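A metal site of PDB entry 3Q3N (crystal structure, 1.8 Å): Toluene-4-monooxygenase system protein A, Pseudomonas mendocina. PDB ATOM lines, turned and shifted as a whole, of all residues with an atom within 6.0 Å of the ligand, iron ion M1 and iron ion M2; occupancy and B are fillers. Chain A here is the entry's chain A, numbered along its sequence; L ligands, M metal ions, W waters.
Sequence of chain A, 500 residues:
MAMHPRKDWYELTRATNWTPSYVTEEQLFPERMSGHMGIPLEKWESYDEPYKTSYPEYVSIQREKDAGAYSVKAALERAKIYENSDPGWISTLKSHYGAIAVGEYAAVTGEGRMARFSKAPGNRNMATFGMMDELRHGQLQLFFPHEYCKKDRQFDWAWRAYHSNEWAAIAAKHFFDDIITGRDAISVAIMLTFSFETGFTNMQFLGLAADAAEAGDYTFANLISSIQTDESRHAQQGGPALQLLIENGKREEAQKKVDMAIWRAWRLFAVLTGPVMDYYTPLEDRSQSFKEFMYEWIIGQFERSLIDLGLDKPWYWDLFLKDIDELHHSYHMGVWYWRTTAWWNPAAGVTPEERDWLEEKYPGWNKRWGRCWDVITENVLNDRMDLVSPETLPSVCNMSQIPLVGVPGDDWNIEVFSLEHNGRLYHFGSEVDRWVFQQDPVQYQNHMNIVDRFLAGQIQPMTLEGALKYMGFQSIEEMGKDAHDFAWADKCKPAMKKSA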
ATOM      1  N   ALA A  99       4.648   6.387  27.204  1.00  0.00           N
ATOM      2  CA  ALA A  99       5.292   6.705  25.924  1.00  0.00           C
ATOM      3  C   ALA A  99       6.706   6.144  25.792  1.00  0.00           C
ATOM      4  O   ALA A  99       7.238   6.049  24.677  1.00  0.00           O
ATOM      5  CB  ALA A  99       5.313   8.208  25.697  1.00  0.00           C
ATOM      6  N   ILE A 100       7.306   5.791  26.931  1.00  0.00           N
ATOM      7  CA  ILE A 100       8.741   5.481  26.989  1.00  0.00           C
ATOM      8  C   ILE A 100       9.096   4.021  27.308  1.00  0.00           C
ATOM      9  O   ILE A 100       9.941   3.428  26.638  1.00  0.00           O
ATOM     10  CB  ILE A 100       9.431   6.381  28.045  1.00  0.00           C
ATOM     11  CG1 ILE A 100       9.372   7.852  27.621  1.00  0.00           C
ATOM     12  CG2 ILE A 100      10.878   5.939  28.286  1.00  0.00           C
ATOM     13  CD1 ILE A 100      10.078   8.161  26.324  1.00  0.00           C
ATOM     14  N   ALA A 101       8.463   3.441  28.322  1.00  0.00           N
ATOM     15  CA  ALA A 101       8.909   2.144  28.847  1.00  0.00           C
ATOM     16  C   ALA A 101       9.123   1.041  27.801  1.00  0.00           C
ATOM     17  O   ALA A 101      10.173   0.402  27.738  1.00  0.00           O
ATOM     18  CB  ALA A 101       7.997   1.655  29.996  1.00  0.00           C
ATOM     19  N   VAL A 102       8.107   0.777  26.984  1.00  0.00           N
ATOM     20  CA  VAL A 102       8.219  -0.312  26.027  1.00  0.00           C
ATOM     21  C   VAL A 102       9.043   0.089  24.791  1.00  0.00           C
ATOM     22  O   VAL A 102       9.564  -0.770  24.088  1.00  0.00           O
ATOM     23  CB  VAL A 102       6.833  -0.922  25.728  1.00  0.00           C
ATOM     24  CG1 VAL A 102       6.898  -1.984  24.628  1.00  0.00           C
ATOM     25  CG2 VAL A 102       6.293  -1.539  27.012  1.00  0.00           C
ATOM     26  N   GLY A 103       9.183   1.398  24.578  1.00  0.00           N
ATOM     27  CA  GLY A 103      10.065   1.919  23.539  1.00  0.00           C
ATOM     28  C   GLY A 103      11.525   1.717  23.915  1.00  0.00           C
ATOM     29  O   GLY A 103      12.359   1.393  23.059  1.00  0.00           O
ATOM     30  N   GLU A 104      11.846   1.900  25.189  1.00  0.00           N
ATOM     31  CA  GLU A 104      13.175   1.582  25.708  1.00  0.00           C
ATOM     32  C   GLU A 104      13.474   0.129  25.393  1.00  0.00           C
ATOM     33  O   GLU A 104      14.570  -0.223  24.964  1.00  0.00           O
ATOM     34  CB  GLU A 104      13.259   1.790  27.230  1.00  0.00           C
ATOM     35  CG  GLU A 104      13.061   3.224  27.686  1.00  0.00           C
ATOM     36  CD  GLU A 104      14.365   3.960  27.867  1.00  0.00           C
ATOM     37  OE1 GLU A 104      14.410   4.940  28.637  1.00  0.00           O
ATOM     38  OE2 GLU A 104      15.350   3.550  27.231  1.00  0.00           O
ATOM     39  N   ALA A 106      12.165  -1.710  23.041  1.00  0.00           N
ATOM     40  CA  ALA A 106      12.385  -1.748  21.603  1.00  0.00           C
ATOM     41  C   ALA A 106      13.805  -1.302  21.236  1.00  0.00           C
ATOM     42  O   ALA A 106      14.417  -1.822  20.312  1.00  0.00           O
ATOM     43  CB  ALA A 106      11.332  -0.887  20.852  1.00  0.00           C
ATOM     44  N   ALA A 107      14.355  -0.327  21.966  1.00  0.00           N
ATOM     45  CA  ALA A 107      15.729   0.116  21.687  1.00  0.00           C
ATOM     46  C   ALA A 107      16.780  -0.986  21.863  1.00  0.00           C
ATOM     47  O   ALA A 107      17.856  -0.908  21.277  1.00  0.00           O
ATOM     48  CB  ALA A 107      16.080   1.340  22.519  1.00  0.00           C
ATOM     49  N   GLU A 111      20.048  -1.654  19.252  1.00  0.00           N
ATOM     50  CA  GLU A 111      21.409  -1.978  19.674  1.00  0.00           C
ATOM     51  C   GLU A 111      21.791  -3.373  19.160  1.00  0.00           C
ATOM     52  O   GLU A 111      22.889  -3.590  18.669  1.00  0.00           O
ATOM     53  CB  GLU A 111      21.519  -1.898  21.211  1.00  0.00           C
ATOM     54  CG  GLU A 111      21.339  -0.451  21.750  1.00  0.00           C
ATOM     55  CD  GLU A 111      22.570   0.432  21.535  1.00  0.00           C
ATOM     56  OE1 GLU A 111      23.614  -0.110  21.157  1.00  0.00           O
ATOM     57  OE2 GLU A 111      22.487   1.667  21.734  1.00  0.00           O
ATOM     58  N   ASP A 133      21.945  -1.862  28.485  1.00  0.00           N
ATOM     59  CA  ASP A 133      21.441  -0.586  28.992  1.00  0.00           C
ATOM     60  C   ASP A 133      19.953  -0.442  28.717  1.00  0.00           C
ATOM     61  O   ASP A 133      19.203  -0.033  29.586  1.00  0.00           O
ATOM     62  CB  ASP A 133      22.142   0.615  28.345  1.00  0.00           C
ATOM     63  CG  ASP A 133      23.599   0.743  28.743  1.00  0.00           C
ATOM     64  OD1 ASP A 133      24.019   0.182  29.788  1.00  0.00           O
ATOM     65  OD2 ASP A 133      24.329   1.459  28.017  1.00  0.00           O
ATOM     66  N   GLU A 134      19.523  -0.704  27.495  1.00  0.00           N
ATOM     67  CA  GLU A 134      18.107  -0.490  27.186  1.00  0.00           C
ATOM     68  C   GLU A 134      17.224  -1.511  27.883  1.00  0.00           C
ATOM     69  O   GLU A 134      16.086  -1.221  28.233  1.00  0.00           O
ATOM     70  CB  GLU A 134      17.849  -0.490  25.673  1.00  0.00           C
ATOM     71  CG  GLU A 134      18.681   0.518  24.882  1.00  0.00           C
ATOM     72  CD  GLU A 134      18.426   1.983  25.264  1.00  0.00           C
ATOM     73  OE1 GLU A 134      17.692   2.290  26.240  1.00  0.00           O
ATOM     74  OE2 GLU A 134      18.998   2.852  24.560  1.00  0.00           O
ATOM     75  N   HIS A 137      16.663   0.015  31.134  1.00  0.00           N
ATOM     76  CA  HIS A 137      15.724   1.130  31.050  1.00  0.00           C
ATOM     77  C   HIS A 137      14.278   0.690  30.921  1.00  0.00           C
ATOM     78  O   HIS A 137      13.404   1.266  31.549  1.00  0.00           O
ATOM     79  CB  HIS A 137      16.105   2.056  29.888  1.00  0.00           C
ATOM     80  CG  HIS A 137      17.489   2.615  30.021  1.00  0.00           C
ATOM     81  ND1 HIS A 137      18.130   3.282  29.006  1.00  0.00           N
ATOM     82  CD2 HIS A 137      18.354   2.594  31.065  1.00  0.00           C
ATOM     83  CE1 HIS A 137      19.342   3.638  29.411  1.00  0.00           C
ATOM     84  NE2 HIS A 137      19.506   3.231  30.655  1.00  0.00           N
ATOM     85  N   GLN A 141      11.485   1.153  33.965  1.00  0.00           N
ATOM     86  CA  GLN A 141      10.324   1.986  33.701  1.00  0.00           C
ATOM     87  C   GLN A 141       9.008   1.217  33.570  1.00  0.00           C
ATOM     88  O   GLN A 141       7.962   1.829  33.375  1.00  0.00           O
ATOM     89  CB  GLN A 141      10.605   2.932  32.538  1.00  0.00           C
ATOM     90  CG  GLN A 141      11.659   3.971  32.936  1.00  0.00           C
ATOM     91  CD  GLN A 141      12.189   4.747  31.762  1.00  0.00           C
ATOM     92  OE1 GLN A 141      12.798   4.181  30.850  1.00  0.00           O
ATOM     93  NE2 GLN A 141      11.981   6.054  31.779  1.00  0.00           N
ATOM     94  N   TYR A 162       2.154   0.585  23.940  1.00  0.00           N
ATOM     95  CA  TYR A 162       2.729   0.112  22.676  1.00  0.00           C
ATOM     96  C   TYR A 162       1.975  -1.074  22.110  1.00  0.00           C
ATOM     97  O   TYR A 162       2.180  -1.465  20.959  1.00  0.00           O
ATOM     98  CB  TYR A 162       4.199  -0.239  22.830  1.00  0.00           C
ATOM     99  CG  TYR A 162       5.112   0.962  22.793  1.00  0.00           C
ATOM    100  CD1 TYR A 162       4.996   1.968  23.742  1.00  0.00           C
ATOM    101  CD2 TYR A 162       6.098   1.091  21.816  1.00  0.00           C
ATOM    102  CE1 TYR A 162       5.829   3.081  23.727  1.00  0.00           C
ATOM    103  CE2 TYR A 162       6.961   2.204  21.800  1.00  0.00           C
ATOM    104  CZ  TYR A 162       6.811   3.193  22.753  1.00  0.00           C
ATOM    105  OH  TYR A 162       7.652   4.295  22.758  1.00  0.00           O
ATOM    106  N   PHE A 176       9.707   5.305  16.490  1.00  0.00           N
ATOM    107  CA  PHE A 176      10.741   4.387  16.961  1.00  0.00           C
ATOM    108  C   PHE A 176      10.982   3.224  16.000  1.00  0.00           C
ATOM    109  O   PHE A 176      12.115   2.758  15.841  1.00  0.00           O
ATOM    110  CB  PHE A 176      10.440   3.899  18.379  1.00  0.00           C
ATOM    111  CG  PHE A 176      10.620   4.971  19.428  1.00  0.00           C
ATOM    112  CD1 PHE A 176      11.772   5.740  19.445  1.00  0.00           C
ATOM    113  CD2 PHE A 176       9.639   5.217  20.370  1.00  0.00           C
ATOM    114  CE1 PHE A 176      11.956   6.727  20.394  1.00  0.00           C
ATOM    115  CE2 PHE A 176       9.805   6.211  21.340  1.00  0.00           C
ATOM    116  CZ  PHE A 176      10.956   6.967  21.350  1.00  0.00           C
ATOM    117  N   ILE A 180      14.689   3.141  15.067  1.00  0.00           N
ATOM    118  CA  ILE A 180      15.291   2.120  15.911  1.00  0.00           C
ATOM    119  C   ILE A 180      15.255   0.710  15.316  1.00  0.00           C
ATOM    120  O   ILE A 180      16.285   0.077  15.133  1.00  0.00           O
ATOM    121  CB  ILE A 180      14.604   2.055  17.290  1.00  0.00           C
ATOM    122  CG1 ILE A 180      14.712   3.412  18.000  1.00  0.00           C
ATOM    123  CG2 ILE A 180      15.208   0.943  18.125  1.00  0.00           C
ATOM    124  CD1 ILE A 180      14.274   3.358  19.481  1.00  0.00           C
ATOM    125  N   LEU A 192      19.487   6.876  15.713  1.00  0.00           N
ATOM    126  CA  LEU A 192      19.230   6.604  17.125  1.00  0.00           C
ATOM    127  C   LEU A 192      20.352   7.135  18.018  1.00  0.00           C
ATOM    128  O   LEU A 192      20.134   8.053  18.819  1.00  0.00           O
ATOM    129  CB  LEU A 192      19.025   5.101  17.349  1.00  0.00           C
ATOM    130  CG  LEU A 192      18.927   4.662  18.814  1.00  0.00           C
ATOM    131  CD1 LEU A 192      17.750   5.336  19.504  1.00  0.00           C
ATOM    132  CD2 LEU A 192      18.815   3.147  18.899  1.00  0.00           C
ATOM    133  N   PHE A 196      18.971  11.074  18.027  1.00  0.00           N
ATOM    134  CA  PHE A 196      18.001  11.008  19.099  1.00  0.00           C
ATOM    135  C   PHE A 196      18.663  10.999  20.477  1.00  0.00           C
ATOM    136  O   PHE A 196      18.251  11.742  21.370  1.00  0.00           O
ATOM    137  CB  PHE A 196      17.137   9.754  18.940  1.00  0.00           C
ATOM    138  CG  PHE A 196      15.960   9.694  19.873  1.00  0.00           C
ATOM    139  CD1 PHE A 196      14.967  10.662  19.815  1.00  0.00           C
ATOM    140  CD2 PHE A 196      15.832   8.662  20.789  1.00  0.00           C
ATOM    141  CE1 PHE A 196      13.876  10.598  20.671  1.00  0.00           C
ATOM    142  CE2 PHE A 196      14.747   8.603  21.650  1.00  0.00           C
ATOM    143  CZ  PHE A 196      13.758   9.576  21.583  1.00  0.00           C
ATOM    144  N   GLU A 197      19.686  10.170  20.649  1.00  0.00           N
ATOM    145  CA  GLU A 197      20.210   9.899  21.990  1.00  0.00           C
ATOM    146  C   GLU A 197      21.249  10.919  22.490  1.00  0.00           C
ATOM    147  O   GLU A 197      21.413  11.083  23.702  1.00  0.00           O
ATOM    148  CB  GLU A 197      20.771   8.473  22.105  1.00  0.00           C
ATOM    149  CG  GLU A 197      19.715   7.363  21.987  1.00  0.00           C
ATOM    150  CD  GLU A 197      20.331   5.965  22.136  1.00  0.00           C
ATOM    151  OE1 GLU A 197      21.481   5.760  21.680  1.00  0.00           O
ATOM    152  OE2 GLU A 197      19.670   5.081  22.720  1.00  0.00           O
ATOM    153  N   THR A 201      16.891  13.178  23.823  1.00  0.00           N
ATOM    154  CA  THR A 201      16.459  12.516  25.063  1.00  0.00           C
ATOM    155  C   THR A 201      16.789  13.349  26.290  1.00  0.00           C
ATOM    156  O   THR A 201      16.080  13.282  27.298  1.00  0.00           O
ATOM    157  CB  THR A 201      17.009  11.097  25.225  1.00  0.00           C
ATOM    158  OG1 THR A 201      18.442  11.118  25.165  1.00  0.00           O
ATOM    159  CG2 THR A 201      16.464  10.186  24.119  1.00  0.00           C
ATOM    160  N   PHE A 205      14.688  13.317  29.887  1.00  0.00           N
ATOM    161  CA  PHE A 205      15.328  12.626  31.000  1.00  0.00           C
ATOM    162  C   PHE A 205      16.154  13.523  31.927  1.00  0.00           C
ATOM    163  O   PHE A 205      16.511  13.125  33.031  1.00  0.00           O
ATOM    164  CB  PHE A 205      16.183  11.458  30.492  1.00  0.00           C
ATOM    165  CG  PHE A 205      15.376  10.319  29.931  1.00  0.00           C
ATOM    166  CD1 PHE A 205      14.870  10.379  28.643  1.00  0.00           C
ATOM    167  CD2 PHE A 205      15.132   9.189  30.688  1.00  0.00           C
ATOM    168  CE1 PHE A 205      14.122   9.327  28.111  1.00  0.00           C
ATOM    169  CE2 PHE A 205      14.382   8.132  30.164  1.00  0.00           C
ATOM    170  CZ  PHE A 205      13.873   8.201  28.892  1.00  0.00           C
ATOM    171  N   ILE A 227      19.187   6.849  34.488  1.00  0.00           N
ATOM    172  CA  ILE A 227      19.030   6.283  33.161  1.00  0.00           C
ATOM    173  C   ILE A 227      19.898   7.032  32.125  1.00  0.00           C
ATOM    174  O   ILE A 227      20.564   6.435  31.287  1.00  0.00           O
ATOM    175  CB  ILE A 227      17.541   6.315  32.761  1.00  0.00           C
ATOM    176  CG1 ILE A 227      16.787   5.179  33.457  1.00  0.00           C
ATOM    177  CG2 ILE A 227      17.385   6.192  31.234  1.00  0.00           C
ATOM    178  CD1 ILE A 227      15.264   5.212  33.244  1.00  0.00           C
ATOM    179  N   ASP A 230      23.528   6.142  31.397  1.00  0.00           N
ATOM    180  CA  ASP A 230      23.790   5.065  30.438  1.00  0.00           C
ATOM    181  C   ASP A 230      23.734   5.604  29.005  1.00  0.00           C
ATOM    182  O   ASP A 230      24.551   5.252  28.142  1.00  0.00           O
ATOM    183  CB  ASP A 230      22.734   3.954  30.542  1.00  0.00           C
ATOM    184  CG  ASP A 230      22.722   3.288  31.900  1.00  0.00           C
ATOM    185  OD1 ASP A 230      23.792   3.078  32.490  1.00  0.00           O
ATOM    186  OD2 ASP A 230      21.608   2.958  32.360  1.00  0.00           O
ATOM    187  N   GLU A 231      22.713   6.423  28.759  1.00  0.00           N
ATOM    188  CA  GLU A 231      22.520   7.034  27.443  1.00  0.00           C
ATOM    189  C   GLU A 231      23.800   7.741  27.041  1.00  0.00           C
ATOM    190  O   GLU A 231      24.270   7.641  25.879  1.00  0.00           O
ATOM    191  CB  GLU A 231      21.367   8.039  27.512  1.00  0.00           C
ATOM    192  CG  GLU A 231      21.052   8.758  26.196  1.00  0.00           C
ATOM    193  CD  GLU A 231      20.035   8.008  25.383  1.00  0.00           C
ATOM    194  OE1 GLU A 231      18.963   8.551  25.074  1.00  0.00           O
ATOM    195  OE2 GLU A 231      20.320   6.838  25.075  1.00  0.00           O
ATOM    196  N   HIS A 234      26.329   5.001  25.719  1.00  0.00           N
ATOM    197  CA  HIS A 234      26.042   4.263  24.472  1.00  0.00           C
ATOM    198  C   HIS A 234      25.669   5.173  23.301  1.00  0.00           C
ATOM    199  O   HIS A 234      25.796   4.768  22.151  1.00  0.00           O
ATOM    200  CB  HIS A 234      25.075   3.089  24.679  1.00  0.00           C
ATOM    201  CG  HIS A 234      23.672   3.464  25.051  1.00  0.00           C
ATOM    202  ND1 HIS A 234      23.052   2.993  26.193  1.00  0.00           N
ATOM    203  CD2 HIS A 234      22.736   4.196  24.393  1.00  0.00           C
ATOM    204  CE1 HIS A 234      21.806   3.437  26.232  1.00  0.00           C
ATOM    205  NE2 HIS A 234      21.594   4.172  25.158  1.00  0.00           N
HETATM  206  C1  LIG L   1      13.569   5.403  24.049  1.00  0.00           C
HETATM  207  C2  LIG L   1      14.009   6.240  25.058  1.00  0.00           C
HETATM  208  C3  LIG L   1      15.354   6.285  25.377  1.00  0.00           C
HETATM  209  C4  LIG L   1      16.257   5.489  24.696  1.00  0.00           C
HETATM  210  C5  LIG L   1      15.817   4.652  23.687  1.00  0.00           C
HETATM  211  C6  LIG L   1      14.472   4.606  23.367  1.00  0.00           C
HETATM  212  O1  LIG L   1      17.599   5.529  25.024  1.00  0.00           O
HETATM  213  N1  LIG L   1      12.183   5.352  23.712  1.00  0.00           N
HETATM  214  O2  LIG L   1      11.774   4.570  22.764  1.00  0.00           O
HETATM  215  O3  LIG L   1      11.382   6.052  24.311  1.00  0.00           O
HETATM  216 FE    FE M   1      19.477   4.947  24.887  1.00  0.00          FE
HETATM  217 FE    FE M   2      17.324   4.144  27.162  1.00  0.00          FE
HETATM  218  O   HOH W   1      16.792   5.935  28.078  1.00  0.00           O
HETATM  219  O   HOH W   2      17.446   8.237  27.295  1.00  0.00           O
HETATM  220  O   HOH W   3      19.268   4.931  26.933  1.00  0.00           O
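Iron ion M2 is bound by OE2 of Glu 104, water W1, OE1 of Glu 134, water W3, ND1 of His 137 and O1 of the ligand.
Of the 25 residues printed, 3 come within 4 Å of iron ion M2. The nearest printed residue that does not touch iron ion M2 is Glu 231 (4.5 Å).
Four residues have an atom within 4 Å of iron ion M1: Glu 134, Glu 197, Glu 231 and His 234.
Iron ion M1 is bound by O1 of the ligand (2.0 Å), water W3 (2.1 Å), OE2 of Glu 231 (2.1 Å), OE2 of Glu 134 (2.2 Å), OE2 of Glu 197 (2.2 Å) and NE2 of His 234 (2.3 Å).
The backbone carbonyl oxygen (O) of Gly 103 lies close to an oxygen (O2) of the ligand, 3.2 Å away. Ile 100 touches the ligand (CD1 to O3, 3.2 Å). Ala 107 touches the ligand (CB to C5, 3.5 Å). Phe 176 touches the ligand (CZ to O2, 2.9 Å). Eight residues have an atom within 4 Å of the ligand: Ile 100, Gly 103, Glu 104, Ala 107, Glu 134, Phe 176, Glu 197 and Glu 231.
NE2 of His 137 is in hydrogen-bond range of O of Ile 227 (3.4 Å). O of Glu 197 sits at hydrogen-bond distance from OG1 of Thr 201 (3.3 Å). A ring nitrogen (ND1) of His 234 sits at hydrogen-bond distance from the backbone carbonyl oxygen (O) of Asp 230, 3.3 Å away. A ring nitrogen (NE2) of His 137 sits close to the backbone carbonyl oxygen of Asp 133, 3.4 Å away. A ring nitrogen (NE2) of His 137 is in hydrogen-bond range of the side-chain carboxylate (OD2) of Asp 230 (2.7 Å). The backbone NH (N) of Glu 197 lies within hydrogen-bond range of the backbone carbonyl oxygen (O) of Leu 192 (2.8 Å). The side-chain carboxylate of Glu 231 lies within hydrogen-bond range of the side-chain hydroxyl of Thr 201 (2.6 Å). The backbone carbonyl oxygen (O) of His 137 lies close to the side-chain amide oxygen (OE1) of Gln 141 (3.1 Å).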
